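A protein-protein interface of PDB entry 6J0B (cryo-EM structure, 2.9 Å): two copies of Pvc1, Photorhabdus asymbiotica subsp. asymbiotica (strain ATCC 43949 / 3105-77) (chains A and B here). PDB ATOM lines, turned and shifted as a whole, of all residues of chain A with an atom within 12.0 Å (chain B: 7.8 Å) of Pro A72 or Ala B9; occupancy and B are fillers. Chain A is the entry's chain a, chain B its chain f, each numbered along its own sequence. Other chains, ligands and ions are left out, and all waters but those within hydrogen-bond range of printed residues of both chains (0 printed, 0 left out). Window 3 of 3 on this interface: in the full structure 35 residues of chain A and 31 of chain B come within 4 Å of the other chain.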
ATOM      1  N   PRO A  29     -11.458   0.453 -39.899  1.00  0.00           N
ATOM      2  CA  PRO A  29     -12.102  -0.861 -39.778  1.00  0.00           C
ATOM      3  C   PRO A  29     -13.557  -0.729 -39.354  1.00  0.00           C
ATOM      4  O   PRO A  29     -13.876  -0.045 -38.381  1.00  0.00           O
ATOM      5  CB  PRO A  29     -11.268  -1.562 -38.704  1.00  0.00           C
ATOM      6  CG  PRO A  29     -10.674  -0.464 -37.916  1.00  0.00           C
ATOM      7  CD  PRO A  29     -10.438   0.664 -38.859  1.00  0.00           C
ATOM      8  N   LYS A  68     -19.874   0.505 -36.689  1.00  0.00           N
ATOM      9  CA  LYS A  68     -18.518   0.550 -36.163  1.00  0.00           C
ATOM     10  C   LYS A  68     -18.564   0.684 -34.650  1.00  0.00           C
ATOM     11  O   LYS A  68     -19.381   1.436 -34.119  1.00  0.00           O
ATOM     12  CB  LYS A  68     -17.758   1.727 -36.771  1.00  0.00           C
ATOM     13  CG  LYS A  68     -16.324   1.851 -36.354  1.00  0.00           C
ATOM     14  CD  LYS A  68     -15.807   3.222 -36.675  1.00  0.00           C
ATOM     15  CE  LYS A  68     -14.364   3.334 -36.283  1.00  0.00           C
ATOM     16  NZ  LYS A  68     -13.598   2.214 -36.867  1.00  0.00           N
ATOM     17  N   GLY A  69     -17.676  -0.034 -33.962  1.00  0.00           N
ATOM     18  CA  GLY A  69     -17.603   0.068 -32.522  1.00  0.00           C
ATOM     19  C   GLY A  69     -16.872   1.311 -32.053  1.00  0.00           C
ATOM     20  O   GLY A  69     -16.089   1.913 -32.779  1.00  0.00           O
ATOM     21  N   VAL A  70     -17.134   1.691 -30.805  1.00  0.00           N
ATOM     22  CA  VAL A  70     -16.571   2.905 -30.220  1.00  0.00           C
ATOM     23  C   VAL A  70     -15.233   2.579 -29.578  1.00  0.00           C
ATOM     24  O   VAL A  70     -15.151   1.730 -28.687  1.00  0.00           O
ATOM     25  CB  VAL A  70     -17.534   3.521 -29.193  1.00  0.00           C
ATOM     26  CG1 VAL A  70     -16.865   4.650 -28.446  1.00  0.00           C
ATOM     27  CG2 VAL A  70     -18.773   4.028 -29.878  1.00  0.00           C
ATOM     28  N   PHE A  71     -14.193   3.265 -30.016  1.00  0.00           N
ATOM     29  CA  PHE A  71     -12.822   3.100 -29.578  1.00  0.00           C
ATOM     30  C   PHE A  71     -12.381   4.328 -28.783  1.00  0.00           C
ATOM     31  O   PHE A  71     -12.874   5.428 -29.040  1.00  0.00           O
ATOM     32  CB  PHE A  71     -11.916   2.875 -30.796  1.00  0.00           C
ATOM     33  CG  PHE A  71     -11.964   1.470 -31.325  1.00  0.00           C
ATOM     34  CD1 PHE A  71     -13.066   1.013 -32.026  1.00  0.00           C
ATOM     35  CD2 PHE A  71     -10.912   0.605 -31.120  1.00  0.00           C
ATOM     36  CE1 PHE A  71     -13.115  -0.274 -32.501  1.00  0.00           C
ATOM     37  CE2 PHE A  71     -10.964  -0.681 -31.606  1.00  0.00           C
ATOM     38  CZ  PHE A  71     -12.064  -1.117 -32.291  1.00  0.00           C
ATOM     39  N   PRO A  72     -11.479   4.177 -27.800  1.00  0.00           N
ATOM     40  CA  PRO A  72     -11.354   5.223 -26.768  1.00  0.00           C
ATOM     41  C   PRO A  72     -10.709   6.516 -27.227  1.00  0.00           C
ATOM     42  O   PRO A  72     -11.045   7.581 -26.698  1.00  0.00           O
ATOM     43  CB  PRO A  72     -10.517   4.532 -25.685  1.00  0.00           C
ATOM     44  CG  PRO A  72      -9.760   3.517 -26.399  1.00  0.00           C
ATOM     45  CD  PRO A  72     -10.666   3.001 -27.452  1.00  0.00           C
ATOM     46  N   GLY A  73      -9.787   6.472 -28.184  1.00  0.00           N
ATOM     47  CA  GLY A  73      -9.168   7.713 -28.600  1.00  0.00           C
ATOM     48  C   GLY A  73      -9.815   8.374 -29.795  1.00  0.00           C
ATOM     49  O   GLY A  73      -9.619   9.574 -30.005  1.00  0.00           O
ATOM     50  N   LYS A  74     -10.605   7.630 -30.561  1.00  0.00           N
ATOM     51  CA  LYS A  74     -10.924   7.978 -31.939  1.00  0.00           C
ATOM     52  C   LYS A  74     -12.405   8.283 -32.095  1.00  0.00           C
ATOM     53  O   LYS A  74     -13.253   7.440 -31.787  1.00  0.00           O
ATOM     54  CB  LYS A  74     -10.533   6.839 -32.888  1.00  0.00           C
ATOM     55  CG  LYS A  74      -9.069   6.827 -33.332  1.00  0.00           C
ATOM     56  CD  LYS A  74      -8.119   6.289 -32.268  1.00  0.00           C
ATOM     57  CE  LYS A  74      -8.563   4.927 -31.754  1.00  0.00           C
ATOM     58  NZ  LYS A  74      -7.722   4.448 -30.619  1.00  0.00           N
ATOM     59  N   THR A  75     -12.714   9.507 -32.554  1.00  0.00           N
ATOM     60  CA  THR A  75     -14.028   9.874 -33.098  1.00  0.00           C
ATOM     61  C   THR A  75     -13.773  10.589 -34.419  1.00  0.00           C
ATOM     62  O   THR A  75     -13.731  11.819 -34.451  1.00  0.00           O
ATOM     63  CB  THR A  75     -14.842  10.794 -32.163  1.00  0.00           C
ATOM     64  OG1 THR A  75     -14.320  12.124 -32.236  1.00  0.00           O
ATOM     65  CG2 THR A  75     -14.783  10.361 -30.739  1.00  0.00           C
ATOM     66  N   GLU A  76     -13.625   9.848 -35.513  1.00  0.00           N
ATOM     67  CA  GLU A  76     -13.573  10.506 -36.810  1.00  0.00           C
ATOM     68  C   GLU A  76     -14.751  10.151 -37.701  1.00  0.00           C
ATOM     69  O   GLU A  76     -14.822  10.637 -38.831  1.00  0.00           O
ATOM     70  CB  GLU A  76     -12.240  10.236 -37.525  1.00  0.00           C
ATOM     71  CG  GLU A  76     -11.888   8.811 -37.886  1.00  0.00           C
ATOM     72  CD  GLU A  76     -10.506   8.739 -38.527  1.00  0.00           C
ATOM     73  OE1 GLU A  76      -9.950   9.808 -38.853  1.00  0.00           O
ATOM     74  OE2 GLU A  76      -9.967   7.629 -38.693  1.00  0.00           O
ATOM     75  N   LEU A  77     -15.684   9.333 -37.215  1.00  0.00           N
ATOM     76  CA  LEU A  77     -17.013   9.308 -37.808  1.00  0.00           C
ATOM     77  C   LEU A  77     -17.850  10.478 -37.322  1.00  0.00           C
ATOM     78  O   LEU A  77     -18.688  10.990 -38.070  1.00  0.00           O
ATOM     79  CB  LEU A  77     -17.737   8.004 -37.479  1.00  0.00           C
ATOM     80  CG  LEU A  77     -17.324   6.709 -38.166  1.00  0.00           C
ATOM     81  CD1 LEU A  77     -18.399   5.662 -37.932  1.00  0.00           C
ATOM     82  CD2 LEU A  77     -17.089   6.930 -39.649  1.00  0.00           C
ATOM     83  N   PHE A  78     -17.643  10.905 -36.077  1.00  0.00           N
ATOM     84  CA  PHE A  78     -18.410  12.014 -35.529  1.00  0.00           C
ATOM     85  C   PHE A  78     -17.936  13.351 -36.079  1.00  0.00           C
ATOM     86  O   PHE A  78     -18.757  14.235 -36.340  1.00  0.00           O
ATOM     87  CB  PHE A  78     -18.330  12.018 -34.003  1.00  0.00           C
ATOM     88  CG  PHE A  78     -18.911  13.251 -33.374  1.00  0.00           C
ATOM     89  CD1 PHE A  78     -18.090  14.246 -32.863  1.00  0.00           C
ATOM     90  CD2 PHE A  78     -20.280  13.422 -33.303  1.00  0.00           C
ATOM     91  CE1 PHE A  78     -18.626  15.382 -32.302  1.00  0.00           C
ATOM     92  CE2 PHE A  78     -20.817  14.555 -32.736  1.00  0.00           C
ATOM     93  CZ  PHE A  78     -19.992  15.535 -32.239  1.00  0.00           C
ATOM     94  N   ASP A  79     -16.621  13.521 -36.242  1.00  0.00           N
ATOM     95  CA  ASP A  79     -16.083  14.792 -36.721  1.00  0.00           C
ATOM     96  C   ASP A  79     -16.455  15.056 -38.171  1.00  0.00           C
ATOM     97  O   ASP A  79     -16.473  16.212 -38.605  1.00  0.00           O
ATOM     98  CB  ASP A  79     -14.565  14.813 -36.570  1.00  0.00           C
ATOM     99  CG  ASP A  79     -14.124  15.114 -35.155  1.00  0.00           C
ATOM    100  OD1 ASP A  79     -14.924  15.687 -34.386  1.00  0.00           O
ATOM    101  OD2 ASP A  79     -12.968  14.792 -34.815  1.00  0.00           O
ATOM    102  N   PRO A 123     -24.421   4.975 -29.285  1.00  0.00           N
ATOM    103  CA  PRO A 123     -24.708   3.687 -28.649  1.00  0.00           C
ATOM    104  C   PRO A 123     -25.813   3.780 -27.614  1.00  0.00           C
ATOM    105  O   PRO A 123     -26.061   4.832 -27.020  1.00  0.00           O
ATOM    106  CB  PRO A 123     -23.377   3.314 -27.990  1.00  0.00           C
ATOM    107  CG  PRO A 123     -22.637   4.591 -27.881  1.00  0.00           C
ATOM    108  CD  PRO A 123     -23.002   5.329 -29.115  1.00  0.00           C
ATOM    109  N   ILE A 132     -20.484  -4.314 -26.878  1.00  0.00           N
ATOM    110  CA  ILE A 132     -19.619  -3.182 -27.163  1.00  0.00           C
ATOM    111  C   ILE A 132     -20.471  -1.991 -27.592  1.00  0.00           C
ATOM    112  O   ILE A 132     -21.541  -2.153 -28.191  1.00  0.00           O
ATOM    113  CB  ILE A 132     -18.625  -3.625 -28.253  1.00  0.00           C
ATOM    114  CG1 ILE A 132     -17.496  -4.405 -27.628  1.00  0.00           C
ATOM    115  CG2 ILE A 132     -18.082  -2.512 -29.139  1.00  0.00           C
ATOM    116  CD1 ILE A 132     -17.432  -5.702 -28.215  1.00  0.00           C
ATOM    117  N   ALA A 133     -20.024  -0.788 -27.237  1.00  0.00           N
ATOM    118  CA  ALA A 133     -20.603   0.436 -27.774  1.00  0.00           C
ATOM    119  C   ALA A 133     -20.366   0.518 -29.274  1.00  0.00           C
ATOM    120  O   ALA A 133     -19.224   0.666 -29.715  1.00  0.00           O
ATOM    121  CB  ALA A 133     -20.003   1.647 -27.071  1.00  0.00           C
ATOM    122  N   VAL A 134     -21.440   0.433 -30.055  1.00  0.00           N
ATOM    123  CA  VAL A 134     -21.358   0.504 -31.507  1.00  0.00           C
ATOM    124  C   VAL A 134     -22.077   1.755 -31.986  1.00  0.00           C
ATOM    125  O   VAL A 134     -22.958   2.288 -31.307  1.00  0.00           O
ATOM    126  CB  VAL A 134     -21.945  -0.748 -32.190  1.00  0.00           C
ATOM    127  CG1 VAL A 134     -20.869  -1.785 -32.407  1.00  0.00           C
ATOM    128  CG2 VAL A 134     -23.067  -1.320 -31.361  1.00  0.00           C
ATOM    129  N   GLN A 135     -21.689   2.219 -33.168  1.00  0.00           N
ATOM    130  CA  GLN A 135     -22.293   3.372 -33.814  1.00  0.00           C
ATOM    131  C   GLN A 135     -22.590   3.049 -35.265  1.00  0.00           C
ATOM    132  O   GLN A 135     -21.746   2.486 -35.962  1.00  0.00           O
ATOM    133  CB  GLN A 135     -21.374   4.578 -33.786  1.00  0.00           C
ATOM    134  CG  GLN A 135     -21.181   5.218 -32.455  1.00  0.00           C
ATOM    135  CD  GLN A 135     -20.188   6.347 -32.540  1.00  0.00           C
ATOM    136  OE1 GLN A 135     -19.162   6.230 -33.208  1.00  0.00           O
ATOM    137  NE2 GLN A 135     -20.495   7.457 -31.882  1.00  0.00           N
ATOM    138  N   THR B   3      -0.958  -9.427 -24.512  1.00  0.00           N
ATOM    139  CA  THR B   3      -1.313  -8.015 -24.513  1.00  0.00           C
ATOM    140  C   THR B   3      -1.137  -7.429 -23.118  1.00  0.00           C
ATOM    141  O   THR B   3      -1.655  -7.968 -22.137  1.00  0.00           O
ATOM    142  CB  THR B   3      -2.753  -7.811 -24.987  1.00  0.00           C
ATOM    143  OG1 THR B   3      -2.987  -8.583 -26.169  1.00  0.00           O
ATOM    144  CG2 THR B   3      -2.991  -6.353 -25.314  1.00  0.00           C
ATOM    145  N   SER B   4      -0.401  -6.326 -23.036  1.00  0.00           N
ATOM    146  CA  SER B   4      -0.241  -5.600 -21.786  1.00  0.00           C
ATOM    147  C   SER B   4      -1.541  -4.894 -21.415  1.00  0.00           C
ATOM    148  O   SER B   4      -2.402  -4.641 -22.258  1.00  0.00           O
ATOM    149  CB  SER B   4       0.897  -4.589 -21.908  1.00  0.00           C
ATOM    150  OG  SER B   4       0.917  -3.704 -20.807  1.00  0.00           O
ATOM    151  N   THR B   5      -1.681  -4.572 -20.129  1.00  0.00           N
ATOM    152  CA  THR B   5      -2.934  -3.990 -19.663  1.00  0.00           C
ATOM    153  C   THR B   5      -3.078  -2.519 -20.027  1.00  0.00           C
ATOM    154  O   THR B   5      -4.196  -1.998 -19.999  1.00  0.00           O
ATOM    155  CB  THR B   5      -3.083  -4.170 -18.150  1.00  0.00           C
ATOM    156  OG1 THR B   5      -4.373  -3.708 -17.740  1.00  0.00           O
ATOM    157  CG2 THR B   5      -2.015  -3.394 -17.398  1.00  0.00           C
ATOM    158  N   SER B   6      -1.986  -1.841 -20.376  1.00  0.00           N
ATOM    159  CA  SER B   6      -2.081  -0.484 -20.889  1.00  0.00           C
ATOM    160  C   SER B   6      -2.295  -0.449 -22.391  1.00  0.00           C
ATOM    161  O   SER B   6      -2.669   0.599 -22.924  1.00  0.00           O
ATOM    162  CB  SER B   6      -0.826   0.315 -20.536  1.00  0.00           C
ATOM    163  OG  SER B   6       0.278  -0.101 -21.316  1.00  0.00           O
ATOM    164  N   GLN B   7      -2.063  -1.566 -23.084  1.00  0.00           N
ATOM    165  CA  GLN B   7      -2.392  -1.638 -24.501  1.00  0.00           C
ATOM    166  C   GLN B   7      -3.892  -1.779 -24.709  1.00  0.00           C
ATOM    167  O   GLN B   7      -4.435  -1.275 -25.697  1.00  0.00           O
ATOM    168  CB  GLN B   7      -1.665  -2.810 -25.157  1.00  0.00           C
ATOM    169  CG  GLN B   7      -0.158  -2.776 -25.045  1.00  0.00           C
ATOM    170  CD  GLN B   7       0.492  -3.878 -25.850  1.00  0.00           C
ATOM    171  OE1 GLN B   7       1.574  -4.358 -25.514  1.00  0.00           O
ATOM    172  NE2 GLN B   7      -0.168  -4.288 -26.924  1.00  0.00           N
ATOM    173  N   ILE B   8      -4.574  -2.470 -23.793  1.00  0.00           N
ATOM    174  CA  ILE B   8      -6.019  -2.653 -23.886  1.00  0.00           C
ATOM    175  C   ILE B   8      -6.744  -1.327 -23.681  1.00  0.00           C
ATOM    176  O   ILE B   8      -7.788  -1.075 -24.297  1.00  0.00           O
ATOM    177  CB  ILE B   8      -6.460  -3.737 -22.880  1.00  0.00           C
ATOM    178  CG1 ILE B   8      -5.780  -5.061 -23.231  1.00  0.00           C
ATOM    179  CG2 ILE B   8      -7.971  -3.917 -22.848  1.00  0.00           C
ATOM    180  CD1 ILE B   8      -6.282  -6.248 -22.469  1.00  0.00           C
ATOM    181  N   ALA B   9      -6.174  -0.431 -22.874  1.00  0.00           N
ATOM    182  CA  ALA B   9      -6.756   0.890 -22.677  1.00  0.00           C
ATOM    183  C   ALA B   9      -6.682   1.759 -23.924  1.00  0.00           C
ATOM    184  O   ALA B   9      -7.449   2.719 -24.036  1.00  0.00           O
ATOM    185  CB  ALA B   9      -6.058   1.601 -21.523  1.00  0.00           C
ATOM    186  N   VAL B  10      -5.790   1.447 -24.858  1.00  0.00           N
ATOM    187  CA  VAL B  10      -5.637   2.246 -26.068  1.00  0.00           C
ATOM    188  C   VAL B  10      -6.314   1.589 -27.266  1.00  0.00           C
ATOM    189  O   VAL B  10      -6.933   2.269 -28.086  1.00  0.00           O
ATOM    190  CB  VAL B  10      -4.139   2.494 -26.331  1.00  0.00           C
ATOM    191  CG1 VAL B  10      -3.945   3.475 -27.469  1.00  0.00           C
ATOM    192  CG2 VAL B  10      -3.467   3.008 -25.079  1.00  0.00           C
ATOM    193  N   GLU B  11      -6.232   0.266 -27.388  1.00  0.00           N
ATOM    194  CA  GLU B  11      -6.658  -0.402 -28.610  1.00  0.00           C
ATOM    195  C   GLU B  11      -8.038  -1.030 -28.535  1.00  0.00           C
ATOM    196  O   GLU B  11      -8.614  -1.319 -29.584  1.00  0.00           O
ATOM    197  CB  GLU B  11      -5.669  -1.502 -28.989  1.00  0.00           C
ATOM    198  CG  GLU B  11      -4.316  -1.008 -29.416  1.00  0.00           C
ATOM    199  CD  GLU B  11      -3.212  -1.939 -28.976  1.00  0.00           C
ATOM    200  OE1 GLU B  11      -3.442  -2.724 -28.035  1.00  0.00           O
ATOM    201  OE2 GLU B  11      -2.116  -1.893 -29.571  1.00  0.00           O
ATOM    202  N   TYR B  12      -8.558  -1.254 -27.387  1.00  0.00           N
ATOM    203  CA  TYR B  12      -9.729  -2.119 -27.370  1.00  0.00           C
ATOM    204  C   TYR B  12     -11.015  -1.302 -27.320  1.00  0.00           C
ATOM    205  O   TYR B  12     -11.019  -0.183 -26.805  1.00  0.00           O
ATOM    206  CB  TYR B  12      -9.664  -3.058 -26.172  1.00  0.00           C
ATOM    207  CG  TYR B  12      -8.928  -4.340 -26.454  1.00  0.00           C
ATOM    208  CD1 TYR B  12      -7.650  -4.327 -26.991  1.00  0.00           C
ATOM    209  CD2 TYR B  12      -9.507  -5.564 -26.177  1.00  0.00           C
ATOM    210  CE1 TYR B  12      -6.977  -5.492 -27.248  1.00  0.00           C
ATOM    211  CE2 TYR B  12      -8.839  -6.735 -26.429  1.00  0.00           C
ATOM    212  CZ  TYR B  12      -7.577  -6.692 -26.965  1.00  0.00           C
ATOM    213  OH  TYR B  12      -6.908  -7.861 -27.220  1.00  0.00           O
ATOM    214  N   PRO B  13     -12.122  -1.828 -27.848  1.00  0.00           N
ATOM    215  CA  PRO B  13     -13.388  -1.093 -27.788  1.00  0.00           C
ATOM    216  C   PRO B  13     -13.919  -0.989 -26.367  1.00  0.00           C
ATOM    217  O   PRO B  13     -13.522  -1.725 -25.464  1.00  0.00           O
ATOM    218  CB  PRO B  13     -14.327  -1.927 -28.660  1.00  0.00           C
ATOM    219  CG  PRO B  13     -13.454  -2.746 -29.496  1.00  0.00           C
ATOM    220  CD  PRO B  13     -12.246  -3.030 -28.688  1.00  0.00           C
ATOM    221  N   ILE B  14     -14.836  -0.054 -26.182  1.00  0.00           N
ATOM    222  CA  ILE B  14     -15.335   0.317 -24.861  1.00  0.00           C
ATOM    223  C   ILE B  14     -16.662  -0.393 -24.623  1.00  0.00           C
ATOM    224  O   ILE B  14     -17.558  -0.296 -25.472  1.00  0.00           O
ATOM    225  CB  ILE B  14     -15.505   1.838 -24.739  1.00  0.00           C
ATOM    226  CG1 ILE B  14     -14.203   2.545 -25.090  1.00  0.00           C
ATOM    227  CG2 ILE B  14     -15.929   2.203 -23.342  1.00  0.00           C
ATOM    228  CD1 ILE B  14     -14.330   4.030 -25.114  1.00  0.00           C
ATOM    229  N   LEU B 106     -12.894   9.021 -17.280  1.00  0.00           N
ATOM    230  CA  LEU B 106     -13.860   8.923 -18.361  1.00  0.00           C
ATOM    231  C   LEU B 106     -13.165   8.460 -19.631  1.00  0.00           C
ATOM    232  O   LEU B 106     -12.005   8.799 -19.877  1.00  0.00           O
ATOM    233  CB  LEU B 106     -14.548  10.260 -18.623  1.00  0.00           C
ATOM    234  CG  LEU B 106     -15.149  11.143 -17.533  1.00  0.00           C
ATOM    235  CD1 LEU B 106     -16.139  12.016 -18.202  1.00  0.00           C
ATOM    236  CD2 LEU B 106     -15.848  10.397 -16.452  1.00  0.00           C
ATOM    237  N   LEU B 107     -13.883   7.691 -20.440  1.00  0.00           N
ATOM    238  CA  LEU B 107     -13.355   7.210 -21.708  1.00  0.00           C
ATOM    239  C   LEU B 107     -13.977   7.921 -22.900  1.00  0.00           C
ATOM    240  O   LEU B 107     -13.266   8.287 -23.837  1.00  0.00           O
ATOM    241  CB  LEU B 107     -13.578   5.700 -21.825  1.00  0.00           C
ATOM    242  CG  LEU B 107     -13.191   4.886 -20.589  1.00  0.00           C
ATOM    243  CD1 LEU B 107     -13.495   3.422 -20.788  1.00  0.00           C
ATOM    244  CD2 LEU B 107     -11.729   5.071 -20.252  1.00  0.00           C
ATOM    245  N   MET B 108     -15.289   8.126 -22.873  1.00  0.00           N
ATOM    246  CA  MET B 108     -16.005   8.906 -23.867  1.00  0.00           C
ATOM    247  C   MET B 108     -17.027   9.764 -23.144  1.00  0.00           C
ATOM    248  O   MET B 108     -17.375   9.498 -21.996  1.00  0.00           O
ATOM    249  CB  MET B 108     -16.703   8.017 -24.894  1.00  0.00           C
ATOM    250  CG  MET B 108     -15.822   7.576 -26.023  1.00  0.00           C
ATOM    251  SD  MET B 108     -15.378   8.956 -27.078  1.00  0.00           S
ATOM    252  CE  MET B 108     -13.959   8.248 -27.885  1.00  0.00           C
ATOM    253  N   THR B 109     -17.501  10.807 -23.817  1.00  0.00           N
ATOM    254  CA  THR B 109     -18.462  11.714 -23.205  1.00  0.00           C
ATOM    255  C   THR B 109     -19.401  12.246 -24.274  1.00  0.00           C
ATOM    256  O   THR B 109     -18.946  12.730 -25.312  1.00  0.00           O
ATOM    257  CB  THR B 109     -17.763  12.879 -22.492  1.00  0.00           C
ATOM    258  OG1 THR B 109     -16.860  12.375 -21.503  1.00  0.00           O
ATOM    259  CG2 THR B 109     -18.772  13.777 -21.802  1.00  0.00           C
ATOM    260  N   MET B 146     -20.230  14.646 -29.127  1.00  0.00           N
ATOM    261  CA  MET B 146     -19.460  13.548 -28.569  1.00  0.00           C
ATOM    262  C   MET B 146     -18.034  14.024 -28.349  1.00  0.00           C
ATOM    263  O   MET B 146     -17.393  14.520 -29.279  1.00  0.00           O
ATOM    264  CB  MET B 146     -19.502  12.345 -29.511  1.00  0.00           C
ATOM    265  CG  MET B 146     -18.523  11.236 -29.229  1.00  0.00           C
ATOM    266  SD  MET B 146     -18.714   9.989 -30.517  1.00  0.00           S
ATOM    267  CE  MET B 146     -17.755   8.632 -29.874  1.00  0.00           C
ATOM    268  N   GLN B 147     -17.552  13.895 -27.122  1.00  0.00           N
ATOM    269  CA  GLN B 147     -16.233  14.376 -26.743  1.00  0.00           C
ATOM    270  C   GLN B 147     -15.316  13.204 -26.443  1.00  0.00           C
ATOM    271  O   GLN B 147     -15.716  12.242 -25.784  1.00  0.00           O
ATOM    272  CB  GLN B 147     -16.308  15.292 -25.523  1.00  0.00           C
ATOM    273  CG  GLN B 147     -16.497  16.755 -25.848  1.00  0.00           C
ATOM    274  CD  GLN B 147     -15.189  17.459 -26.157  1.00  0.00           C
ATOM    275  OE1 GLN B 147     -14.120  16.849 -26.136  1.00  0.00           O
ATOM    276  NE2 GLN B 147     -15.269  18.752 -26.439  1.00  0.00           N
ATOM    277  N   ALA B 148     -14.084  13.289 -26.928  1.00  0.00           N
ATOM    278  CA  ALA B 148     -13.092  12.276 -26.608  1.00  0.00           C
ATOM    279  C   ALA B 148     -12.550  12.513 -25.207  1.00  0.00           C
ATOM    280  O   ALA B 148     -12.046  13.600 -24.906  1.00  0.00           O
ATOM    281  CB  ALA B 148     -11.957  12.299 -27.627  1.00  0.00           C
ATOM    282  N   VAL B 149     -12.671  11.488 -24.360  1.00  0.00           N
ATOM    283  CA  VAL B 149     -12.217  11.470 -22.963  1.00  0.00           C
ATOM    284  C   VAL B 149     -12.802  12.612 -22.135  1.00  0.00           C
ATOM    285  O   VAL B 149     -14.006  12.653 -21.881  1.00  0.00           O
ATOM    286  CB  VAL B 149     -10.676  11.476 -22.878  1.00  0.00           C
ATOM    287  CG1 VAL B 149     -10.235  11.261 -21.457  1.00  0.00           C
ATOM    288  CG2 VAL B 149     -10.087  10.401 -23.776  1.00  0.00           C
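The backbone NH (N) of Ile B14 is in hydrogen-bond range of the backbone carbonyl oxygen (O) of Val A70. The side-chain amino group (NZ) of Lys A74 sits at hydrogen-bond distance from the backbone carbonyl oxygen (O) of Val B10 (3.4 Å). N of Ala A133 sits at hydrogen-bond distance from O of Ile B14 (3.1 Å). The side-chain amide nitrogen (NE2) of Gln A135 sits at hydrogen-bond distance from the side-chain sulfur (SD) of Met B146 (3.4 Å).
The backbone carbonyl oxygen (O) of Ala A133 lies within hydrogen-bond range of the backbone NH (N) of Val A70. The backbone carbonyl oxygen of Leu B107 is in hydrogen-bond range of the backbone NH of Val B149 (3.3 Å). O of Lys A68 is in hydrogen-bond range of N of Gln A135, 2.6 Å away.
Val A70 touches Met B108. CG of Pro B13 touches CZ of Phe A71, 3.5 Å away. Phe A71 touches Met B108. CG of Pro A72 touches O of Val B10, 3.5 Å away. CA of Pro A72 touches CD1 of Ile B14, 3.6 Å away. Leu B107 touches Pro A72. Thr A75 touches Met B108. Met B146 touches Thr A75. N of Met B146 touches CZ of Phe A78, at 3.2 Å. Ile A132 touches Ile B14 (CA to O, 3.9 Å).
Pro A29 touches none of the printed residues of chain B. Printed residues of chain B within 4 Å of Val A70: Pro B13 (3.4 Å), Ile B14 (3.1 Å) and Met B108 (3.9 Å). Pro A72 touches just these residues of chain B: Ala B9, Val B10, Tyr B12, Ile B14, Leu B107 and Met B108. Printed residues of chain B within 4 Å of Thr A75: Met B108 (3.6 Å) and Met B146 (3.5 Å). Glu A76 touches none of the printed residues of chain B. Of the printed residues of chain B, Phe A78 touches Met B146 (3.2 Å). No residue of chain A comes within 4 Å of Thr B5. No residue of chain A comes within 4 Å of Ser B6. No residue of chain A comes within 4 Å of Ile B8. Printed residues of chain A within 4 Å of Ala B9: Pro A72. Val B10 touches two residues of chain A. Leu B107 touches just one residue of chain A: Pro A72 (3.7 Å). Printed residues of chain A within 4 Å of Met B146: Thr A75 (3.5 Å), Phe A78 (3.2 Å) and Gln A135 (3.4 Å). No residue of chain A comes within 4 Å of Ala B148. The nearest residue of chain A that does not touch Ala B9 is Gly A73 (6.1 Å).
Hydrophobic or aromatic side chains of chain A that line the printed part of chain B: Val A70, Phe A71, Pro A72, Phe A78, Ile A132 and Ala A133. Of the 20 printed residues of chain B, 9 touch a printed residue of chain A. Printed residues of chain B that touch a printed residue of chain A: Ala B9, Val B10, Glu B11, Tyr B12, Pro B13, Ile B14, Leu B107, Met B108 and Met B146. Hydrophobic or aromatic side chains of chain B that line the printed part of chain A: Pro B13, Ile B14, Met B108 and Met B146. Among the printed residues, 20 pairs touch across the chains.
No position is printed for both chains. Of the 20 pairs that touch across the chains among the printed residues, none has its exchanged pair printed and touching as well.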
